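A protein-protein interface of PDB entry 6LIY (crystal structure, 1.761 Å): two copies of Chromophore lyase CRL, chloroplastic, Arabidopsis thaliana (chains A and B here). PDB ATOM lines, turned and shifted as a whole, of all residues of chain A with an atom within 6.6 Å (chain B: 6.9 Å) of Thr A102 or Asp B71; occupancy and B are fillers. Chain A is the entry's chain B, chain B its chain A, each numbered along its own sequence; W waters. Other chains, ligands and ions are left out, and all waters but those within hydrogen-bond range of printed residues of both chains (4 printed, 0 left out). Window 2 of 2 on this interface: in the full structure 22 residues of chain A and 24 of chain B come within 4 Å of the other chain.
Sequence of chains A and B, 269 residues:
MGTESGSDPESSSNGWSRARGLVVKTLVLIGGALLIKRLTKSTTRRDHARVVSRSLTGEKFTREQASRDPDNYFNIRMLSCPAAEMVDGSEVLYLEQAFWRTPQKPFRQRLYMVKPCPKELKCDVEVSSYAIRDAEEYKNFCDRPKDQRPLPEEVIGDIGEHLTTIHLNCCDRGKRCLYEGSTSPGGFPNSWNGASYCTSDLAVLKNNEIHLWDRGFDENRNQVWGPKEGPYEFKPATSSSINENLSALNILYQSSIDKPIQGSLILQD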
ATOM      1  N   ALA A  98     -22.304   9.697   6.049  1.00  0.00           N
ATOM      2  CA  ALA A  98     -21.741  10.574   7.064  1.00  0.00           C
ATOM      3  C   ALA A  98     -20.277  10.223   7.269  1.00  0.00           C
ATOM      4  O   ALA A  98     -19.863   9.079   7.076  1.00  0.00           O
ATOM      5  CB  ALA A  98     -22.491  10.456   8.392  1.00  0.00           C
ATOM      6  N   PHE A  99     -19.491  11.224   7.661  1.00  0.00           N
ATOM      7  CA  PHE A  99     -18.148  10.936   8.140  1.00  0.00           C
ATOM      8  C   PHE A  99     -18.244  10.092   9.402  1.00  0.00           C
ATOM      9  O   PHE A  99     -19.091  10.338  10.262  1.00  0.00           O
ATOM     10  CB  PHE A  99     -17.420  12.251   8.427  1.00  0.00           C
ATOM     11  CG  PHE A  99     -15.978  12.092   8.813  1.00  0.00           C
ATOM     12  CD1 PHE A  99     -15.127  11.297   8.063  1.00  0.00           C
ATOM     13  CD2 PHE A  99     -15.466  12.769   9.912  1.00  0.00           C
ATOM     14  CE1 PHE A  99     -13.793  11.169   8.414  1.00  0.00           C
ATOM     15  CE2 PHE A  99     -14.140  12.640  10.266  1.00  0.00           C
ATOM     16  CZ  PHE A  99     -13.306  11.835   9.514  1.00  0.00           C
ATOM     17  N   TRP A 100     -17.344   9.118   9.537  1.00  0.00           N
ATOM     18  CA  TRP A 100     -17.501   8.140  10.613  1.00  0.00           C
ATOM     19  C   TRP A 100     -17.459   8.781  12.001  1.00  0.00           C
ATOM     20  O   TRP A 100     -18.052   8.248  12.949  1.00  0.00           O
ATOM     21  CB  TRP A 100     -16.432   7.051  10.503  1.00  0.00           C
ATOM     22  CG  TRP A 100     -15.080   7.481  10.954  1.00  0.00           C
ATOM     23  CD1 TRP A 100     -14.167   8.213  10.244  1.00  0.00           C
ATOM     24  CD2 TRP A 100     -14.472   7.206  12.222  1.00  0.00           C
ATOM     25  NE1 TRP A 100     -13.028   8.395  10.989  1.00  0.00           N
ATOM     26  CE2 TRP A 100     -13.192   7.797  12.208  1.00  0.00           C
ATOM     27  CE3 TRP A 100     -14.884   6.518  13.363  1.00  0.00           C
ATOM     28  CZ2 TRP A 100     -12.322   7.734  13.302  1.00  0.00           C
ATOM     29  CZ3 TRP A 100     -14.021   6.450  14.448  1.00  0.00           C
ATOM     30  CH2 TRP A 100     -12.753   7.057  14.405  1.00  0.00           C
ATOM     31  N   ARG A 101     -16.765   9.917  12.144  1.00  0.00           N
ATOM     32  CA  ARG A 101     -16.676  10.589  13.436  1.00  0.00           C
ATOM     33  C   ARG A 101     -17.916  11.413  13.767  1.00  0.00           C
ATOM     34  O   ARG A 101     -18.086  11.816  14.925  1.00  0.00           O
ATOM     35  CB  ARG A 101     -15.449  11.511  13.473  1.00  0.00           C
ATOM     36  CG  ARG A 101     -14.124  10.780  13.366  1.00  0.00           C
ATOM     37  CD  ARG A 101     -12.962  11.737  13.595  1.00  0.00           C
ATOM     38  NE  ARG A 101     -12.757  11.994  15.019  1.00  0.00           N
ATOM     39  CZ  ARG A 101     -11.627  11.724  15.671  1.00  0.00           C
ATOM     40  NH1 ARG A 101     -10.594  11.193  15.029  1.00  0.00           N
ATOM     41  NH2 ARG A 101     -11.533  11.984  16.966  1.00  0.00           N
ATOM     42  N   THR A 102     -18.771  11.702  12.784  1.00  0.00           N
ATOM     43  CA  THR A 102     -19.993  12.477  13.007  1.00  0.00           C
ATOM     44  C   THR A 102     -21.182  11.767  12.366  1.00  0.00           C
ATOM     45  O   THR A 102     -21.847  12.316  11.483  1.00  0.00           O
ATOM     46  CB  THR A 102     -19.849  13.895  12.456  1.00  0.00           C
ATOM     47  OG1 THR A 102     -19.457  13.843  11.076  1.00  0.00           O
ATOM     48  CG2 THR A 102     -18.798  14.684  13.253  1.00  0.00           C
ATOM     49  N   PRO A 103     -21.485  10.544  12.808  1.00  0.00           N
ATOM     50  CA  PRO A 103     -22.571   9.780  12.171  1.00  0.00           C
ATOM     51  C   PRO A 103     -23.920  10.453  12.301  1.00  0.00           C
ATOM     52  O   PRO A 103     -24.826  10.172  11.509  1.00  0.00           O
ATOM     53  CB  PRO A 103     -22.534   8.437  12.914  1.00  0.00           C
ATOM     54  CG  PRO A 103     -21.928   8.773  14.259  1.00  0.00           C
ATOM     55  CD  PRO A 103     -20.901   9.821  13.959  1.00  0.00           C
ATOM     56  N   GLN A 104     -24.072  11.350  13.266  1.00  0.00           N
ATOM     57  CA  GLN A 104     -25.316  12.064  13.481  1.00  0.00           C
ATOM     58  C   GLN A 104     -25.477  13.271  12.565  1.00  0.00           C
ATOM     59  O   GLN A 104     -26.536  13.904  12.591  1.00  0.00           O
ATOM     60  CB  GLN A 104     -25.395  12.503  14.951  1.00  0.00           C
ATOM     61  CG  GLN A 104     -24.495  13.691  15.320  1.00  0.00           C
ATOM     62  CD  GLN A 104     -23.042  13.321  15.639  1.00  0.00           C
ATOM     63  OE1 GLN A 104     -22.508  12.320  15.161  1.00  0.00           O
ATOM     64  NE2 GLN A 104     -22.397  14.152  16.440  1.00  0.00           N
ATOM     65  N   LYS A 105     -24.461  13.629  11.782  1.00  0.00           N
ATOM     66  CA  LYS A 105     -24.491  14.827  10.941  1.00  0.00           C
ATOM     67  C   LYS A 105     -24.153  14.430   9.512  1.00  0.00           C
ATOM     68  O   LYS A 105     -23.083  14.772   8.990  1.00  0.00           O
ATOM     69  CB  LYS A 105     -23.522  15.908  11.432  1.00  0.00           C
ATOM     70  CG  LYS A 105     -23.483  16.148  12.928  1.00  0.00           C
ATOM     71  CD  LYS A 105     -22.651  17.408  13.224  1.00  0.00           C
ATOM     72  CE  LYS A 105     -21.794  17.249  14.466  1.00  0.00           C
ATOM     73  NZ  LYS A 105     -20.838  18.393  14.626  1.00  0.00           N
ATOM     74  N   PRO A 106     -25.053  13.714   8.844  1.00  0.00           N
ATOM     75  CA  PRO A 106     -24.768  13.263   7.480  1.00  0.00           C
ATOM     76  C   PRO A 106     -24.535  14.435   6.545  1.00  0.00           C
ATOM     77  O   PRO A 106     -25.167  15.484   6.673  1.00  0.00           O
ATOM     78  CB  PRO A 106     -26.036  12.493   7.093  1.00  0.00           C
ATOM     79  CG  PRO A 106     -27.110  13.065   7.965  1.00  0.00           C
ATOM     80  CD  PRO A 106     -26.435  13.406   9.259  1.00  0.00           C
ATOM     81  N   PHE A 107     -23.611  14.245   5.606  1.00  0.00           N
ATOM     82  CA  PHE A 107     -23.306  15.259   4.611  1.00  0.00           C
ATOM     83  C   PHE A 107     -24.088  15.055   3.327  1.00  0.00           C
ATOM     84  O   PHE A 107     -24.076  15.938   2.467  1.00  0.00           O
ATOM     85  CB  PHE A 107     -21.800  15.293   4.301  1.00  0.00           C
ATOM     86  CG  PHE A 107     -21.263  14.028   3.652  1.00  0.00           C
ATOM     87  CD1 PHE A 107     -21.279  13.884   2.271  1.00  0.00           C
ATOM     88  CD2 PHE A 107     -20.725  13.006   4.421  1.00  0.00           C
ATOM     89  CE1 PHE A 107     -20.794  12.730   1.662  1.00  0.00           C
ATOM     90  CE2 PHE A 107     -20.233  11.827   3.806  1.00  0.00           C
ATOM     91  CZ  PHE A 107     -20.260  11.700   2.440  1.00  0.00           C
ATOM     92  N   ALA B  66      -7.214  20.854  12.887  1.00  0.00           N
ATOM     93  CA  ALA B  66      -7.554  19.444  12.710  1.00  0.00           C
ATOM     94  C   ALA B  66      -7.147  18.621  13.925  1.00  0.00           C
ATOM     95  O   ALA B  66      -7.810  17.634  14.254  1.00  0.00           O
ATOM     96  CB  ALA B  66      -6.880  18.896  11.457  1.00  0.00           C
ATOM     97  N   ARG B  68      -7.137  19.894  16.980  1.00  0.00           N
ATOM     98  CA  ARG B  68      -8.017  20.342  18.051  1.00  0.00           C
ATOM     99  C   ARG B  68      -9.409  19.733  17.928  1.00  0.00           C
ATOM    100  O   ARG B  68     -10.029  19.387  18.937  1.00  0.00           O
ATOM    101  CB  ARG B  68      -8.094  21.866  18.037  1.00  0.00           C
ATOM    102  CG  ARG B  68      -9.021  22.478  19.065  1.00  0.00           C
ATOM    103  CD  ARG B  68      -8.927  24.002  19.060  1.00  0.00           C
ATOM    104  NE  ARG B  68      -9.675  24.605  17.957  1.00  0.00           N
ATOM    105  CZ  ARG B  68      -9.123  25.251  16.933  1.00  0.00           C
ATOM    106  NH1 ARG B  68      -7.807  25.385  16.848  1.00  0.00           N
ATOM    107  NH2 ARG B  68      -9.893  25.760  15.985  1.00  0.00           N
ATOM    108  N   ASP B  69      -9.916  19.580  16.700  1.00  0.00           N
ATOM    109  CA  ASP B  69     -11.299  19.160  16.465  1.00  0.00           C
ATOM    110  C   ASP B  69     -11.347  18.209  15.276  1.00  0.00           C
ATOM    111  O   ASP B  69     -11.927  18.523  14.227  1.00  0.00           O
ATOM    112  CB  ASP B  69     -12.182  20.387  16.228  1.00  0.00           C
ATOM    113  CG  ASP B  69     -13.667  20.079  16.258  1.00  0.00           C
ATOM    114  OD1 ASP B  69     -14.041  18.911  16.469  1.00  0.00           O
ATOM    115  OD2 ASP B  69     -14.454  21.037  16.058  1.00  0.00           O
ATOM    116  N   PRO B  70     -10.753  17.019  15.413  1.00  0.00           N
ATOM    117  CA  PRO B  70     -10.684  16.093  14.269  1.00  0.00           C
ATOM    118  C   PRO B  70     -12.039  15.583  13.821  1.00  0.00           C
ATOM    119  O   PRO B  70     -12.163  15.128  12.677  1.00  0.00           O
ATOM    120  CB  PRO B  70      -9.813  14.951  14.795  1.00  0.00           C
ATOM    121  CG  PRO B  70     -10.055  14.970  16.278  1.00  0.00           C
ATOM    122  CD  PRO B  70     -10.166  16.430  16.635  1.00  0.00           C
ATOM    123  N   ASP B  71     -13.057  15.647  14.680  1.00  0.00           N
ATOM    124  CA  ASP B  71     -14.400  15.252  14.275  1.00  0.00           C
ATOM    125  C   ASP B  71     -14.908  16.099  13.117  1.00  0.00           C
ATOM    126  O   ASP B  71     -15.659  15.609  12.266  1.00  0.00           O
ATOM    127  CB  ASP B  71     -15.383  15.408  15.436  1.00  0.00           C
ATOM    128  CG  ASP B  71     -15.277  14.308  16.465  1.00  0.00           C
ATOM    129  OD1 ASP B  71     -14.472  13.366  16.305  1.00  0.00           O
ATOM    130  OD2 ASP B  71     -16.021  14.414  17.456  1.00  0.00           O
ATOM    131  N   ASN B  72     -14.535  17.369  13.076  1.00  0.00           N
ATOM    132  CA  ASN B  72     -15.186  18.317  12.191  1.00  0.00           C
ATOM    133  C   ASN B  72     -14.273  18.968  11.170  1.00  0.00           C
ATOM    134  O   ASN B  72     -14.784  19.619  10.256  1.00  0.00           O
ATOM    135  CB  ASN B  72     -15.860  19.428  13.010  1.00  0.00           C
ATOM    136  CG  ASN B  72     -16.937  18.887  13.909  1.00  0.00           C
ATOM    137  OD1 ASN B  72     -17.929  18.332  13.435  1.00  0.00           O
ATOM    138  ND2 ASN B  72     -16.736  19.010  15.223  1.00  0.00           N
ATOM    139  N   TYR B  73     -12.957  18.831  11.291  1.00  0.00           N
ATOM    140  CA  TYR B  73     -12.046  19.506  10.375  1.00  0.00           C
ATOM    141  C   TYR B  73     -10.879  18.608  10.011  1.00  0.00           C
ATOM    142  O   TYR B  73     -10.314  17.925  10.872  1.00  0.00           O
ATOM    143  CB  TYR B  73     -11.504  20.803  10.980  1.00  0.00           C
ATOM    144  CG  TYR B  73     -12.593  21.769  11.346  1.00  0.00           C
ATOM    145  CD1 TYR B  73     -13.152  22.606  10.394  1.00  0.00           C
ATOM    146  CD2 TYR B  73     -13.077  21.838  12.645  1.00  0.00           C
ATOM    147  CE1 TYR B  73     -14.161  23.482  10.735  1.00  0.00           C
ATOM    148  CE2 TYR B  73     -14.083  22.721  12.993  1.00  0.00           C
ATOM    149  CZ  TYR B  73     -14.622  23.538  12.029  1.00  0.00           C
ATOM    150  OH  TYR B  73     -15.625  24.421  12.361  1.00  0.00           O
ATOM    151  N   PHE B  74     -10.508  18.642   8.740  1.00  0.00           N
ATOM    152  CA  PHE B  74      -9.355  17.920   8.230  1.00  0.00           C
ATOM    153  C   PHE B  74      -8.154  18.850   8.131  1.00  0.00           C
ATOM    154  O   PHE B  74      -8.271  20.073   8.223  1.00  0.00           O
ATOM    155  CB  PHE B  74      -9.672  17.310   6.856  1.00  0.00           C
ATOM    156  CG  PHE B  74     -10.830  16.369   6.880  1.00  0.00           C
ATOM    157  CD1 PHE B  74     -10.649  15.049   7.253  1.00  0.00           C
ATOM    158  CD2 PHE B  74     -12.106  16.806   6.561  1.00  0.00           C
ATOM    159  CE1 PHE B  74     -11.717  14.159   7.281  1.00  0.00           C
ATOM    160  CE2 PHE B  74     -13.192  15.925   6.594  1.00  0.00           C
ATOM    161  CZ  PHE B  74     -12.990  14.596   6.956  1.00  0.00           C
ATOM    162  N   LYS B 228     -19.687  21.962   8.037  1.00  0.00           N
ATOM    163  CA  LYS B 228     -20.912  22.345   8.724  1.00  0.00           C
ATOM    164  C   LYS B 228     -20.672  23.225   9.939  1.00  0.00           C
ATOM    165  O   LYS B 228     -21.541  24.030  10.290  1.00  0.00           O
ATOM    166  CB  LYS B 228     -21.676  21.096   9.171  1.00  0.00           C
ATOM    167  CG  LYS B 228     -21.981  20.141   8.041  1.00  0.00           C
ATOM    168  CD  LYS B 228     -22.378  18.769   8.590  1.00  0.00           C
ATOM    169  CE  LYS B 228     -23.080  17.950   7.534  1.00  0.00           C
ATOM    170  NZ  LYS B 228     -24.169  18.741   6.861  1.00  0.00           N
ATOM    171  N   GLU B 229     -19.525  23.087  10.600  1.00  0.00           N
ATOM    172  CA  GLU B 229     -19.392  23.647  11.939  1.00  0.00           C
ATOM    173  C   GLU B 229     -18.912  25.088  11.950  1.00  0.00           C
ATOM    174  O   GLU B 229     -19.266  25.843  12.862  1.00  0.00           O
ATOM    175  CB  GLU B 229     -18.432  22.792  12.763  1.00  0.00           C
ATOM    176  CG  GLU B 229     -18.986  21.407  13.062  1.00  0.00           C
ATOM    177  CD  GLU B 229     -20.318  21.460  13.780  1.00  0.00           C
ATOM    178  OE1 GLU B 229     -20.362  22.042  14.885  1.00  0.00           O
ATOM    179  OE2 GLU B 229     -21.316  20.909  13.249  1.00  0.00           O
HETATM  180  O   HOH W   1     -19.245  13.720  16.913  1.00  0.00           O
HETATM  181  O   HOH W   2     -17.797  15.844  10.281  1.00  0.00           O
HETATM  182  O   HOH W   3     -23.470  18.628   3.531  1.00  0.00           O
HETATM  183  O   HOH W   4     -26.499  16.939   8.595  1.00  0.00           O
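The side-chain amide oxygen (OD1) of Asn B72 lies within hydrogen-bond range of the side-chain amino group (NZ) of Lys A105. The side-chain carboxylate of Glu B229 lies within salt-bridge range of the side-chain amino group of Lys A105 (2.9 Å). O of Pro A106 sits close to NZ of Lys B228 (3.4 Å). NE of Arg A101 is in salt-bridge range of OD1 of Asp B71, at 2.5 Å.
The side-chain carboxylate (OD1) of Asp B69 lies within hydrogen-bond range of the side-chain amide nitrogen (ND2) of Asn B72 (3.0 Å).
Among the printed residues, pairs that only touch across the chains: Phe A99 with Pro B70 (3.99 Å), Phe A99 with Asp B71 (3.7 Å), Phe A99 with Phe B74 (3.6 Å), Arg A101 with Pro B70 (3.4 Å), Thr A102 with Asp B71 (3.4 Å), Thr A102 with Asn B72 (3.8 Å), Lys A105 with Lys B228 (3.5 Å) and Phe A107 with Lys B228 (3.98 Å).
Of the printed residues of chain B, Lys A105 touches Asn B72 (3.1 Å), Lys B228 (3.5 Å) and Glu B229 (2.9 Å). Of the printed residues of chain B, Arg A101 touches Pro B70 and Asp B71. Printed residues of chain A within 4 Å of Phe B74: Phe A99 (3.6 Å). Trp A100 touches none of the printed residues of chain B. The nearest residue of chain A that does not touch Asp B71 is Lys A105 (6.3 Å). The nearest printed residue of chain A that does not touch Phe B74 is Arg A101 (6.9 Å).
Printed residues of chain B that touch a printed residue of chain A: Pro B70, Asp B71, Asn B72, Phe B74, Lys B228 and Glu B229. Hydrophobic or aromatic side chains of chain A that line the printed part of chain B: Phe A99. Among the printed residues, Asp or Glu carboxylates within 4 Å of a Lys or Arg side-chain nitrogen of the other chain: Arg A101 with Asp B71 (2.5 Å) and Lys A105 with Glu B229 (2.9 Å).
No position is printed for both chains. Of the 12 pairs that touch across the chains among the printed residues, none has its exchanged pair printed and touching as well.
Water W2 lies within hydrogen-bond range of OG1 of Thr A102 and O of Asp B71. Water W4 lies within hydrogen-bond range of O of Pro A106 (2.8 Å) and NZ of Lys B228 (3.4 Å). Water W3 bridges the backbone carbonyl oxygen (O) of Phe A107 (3.0 Å) and the side-chain amino group (NZ) of Lys B228 (3.4 Å). Water W1 lies within hydrogen-bond range of the backbone carbonyl oxygen (O) of Arg A101, the side-chain amide nitrogen (NE2) of Gln A104 and the side-chain carboxylate (OD2) of Asp B71.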
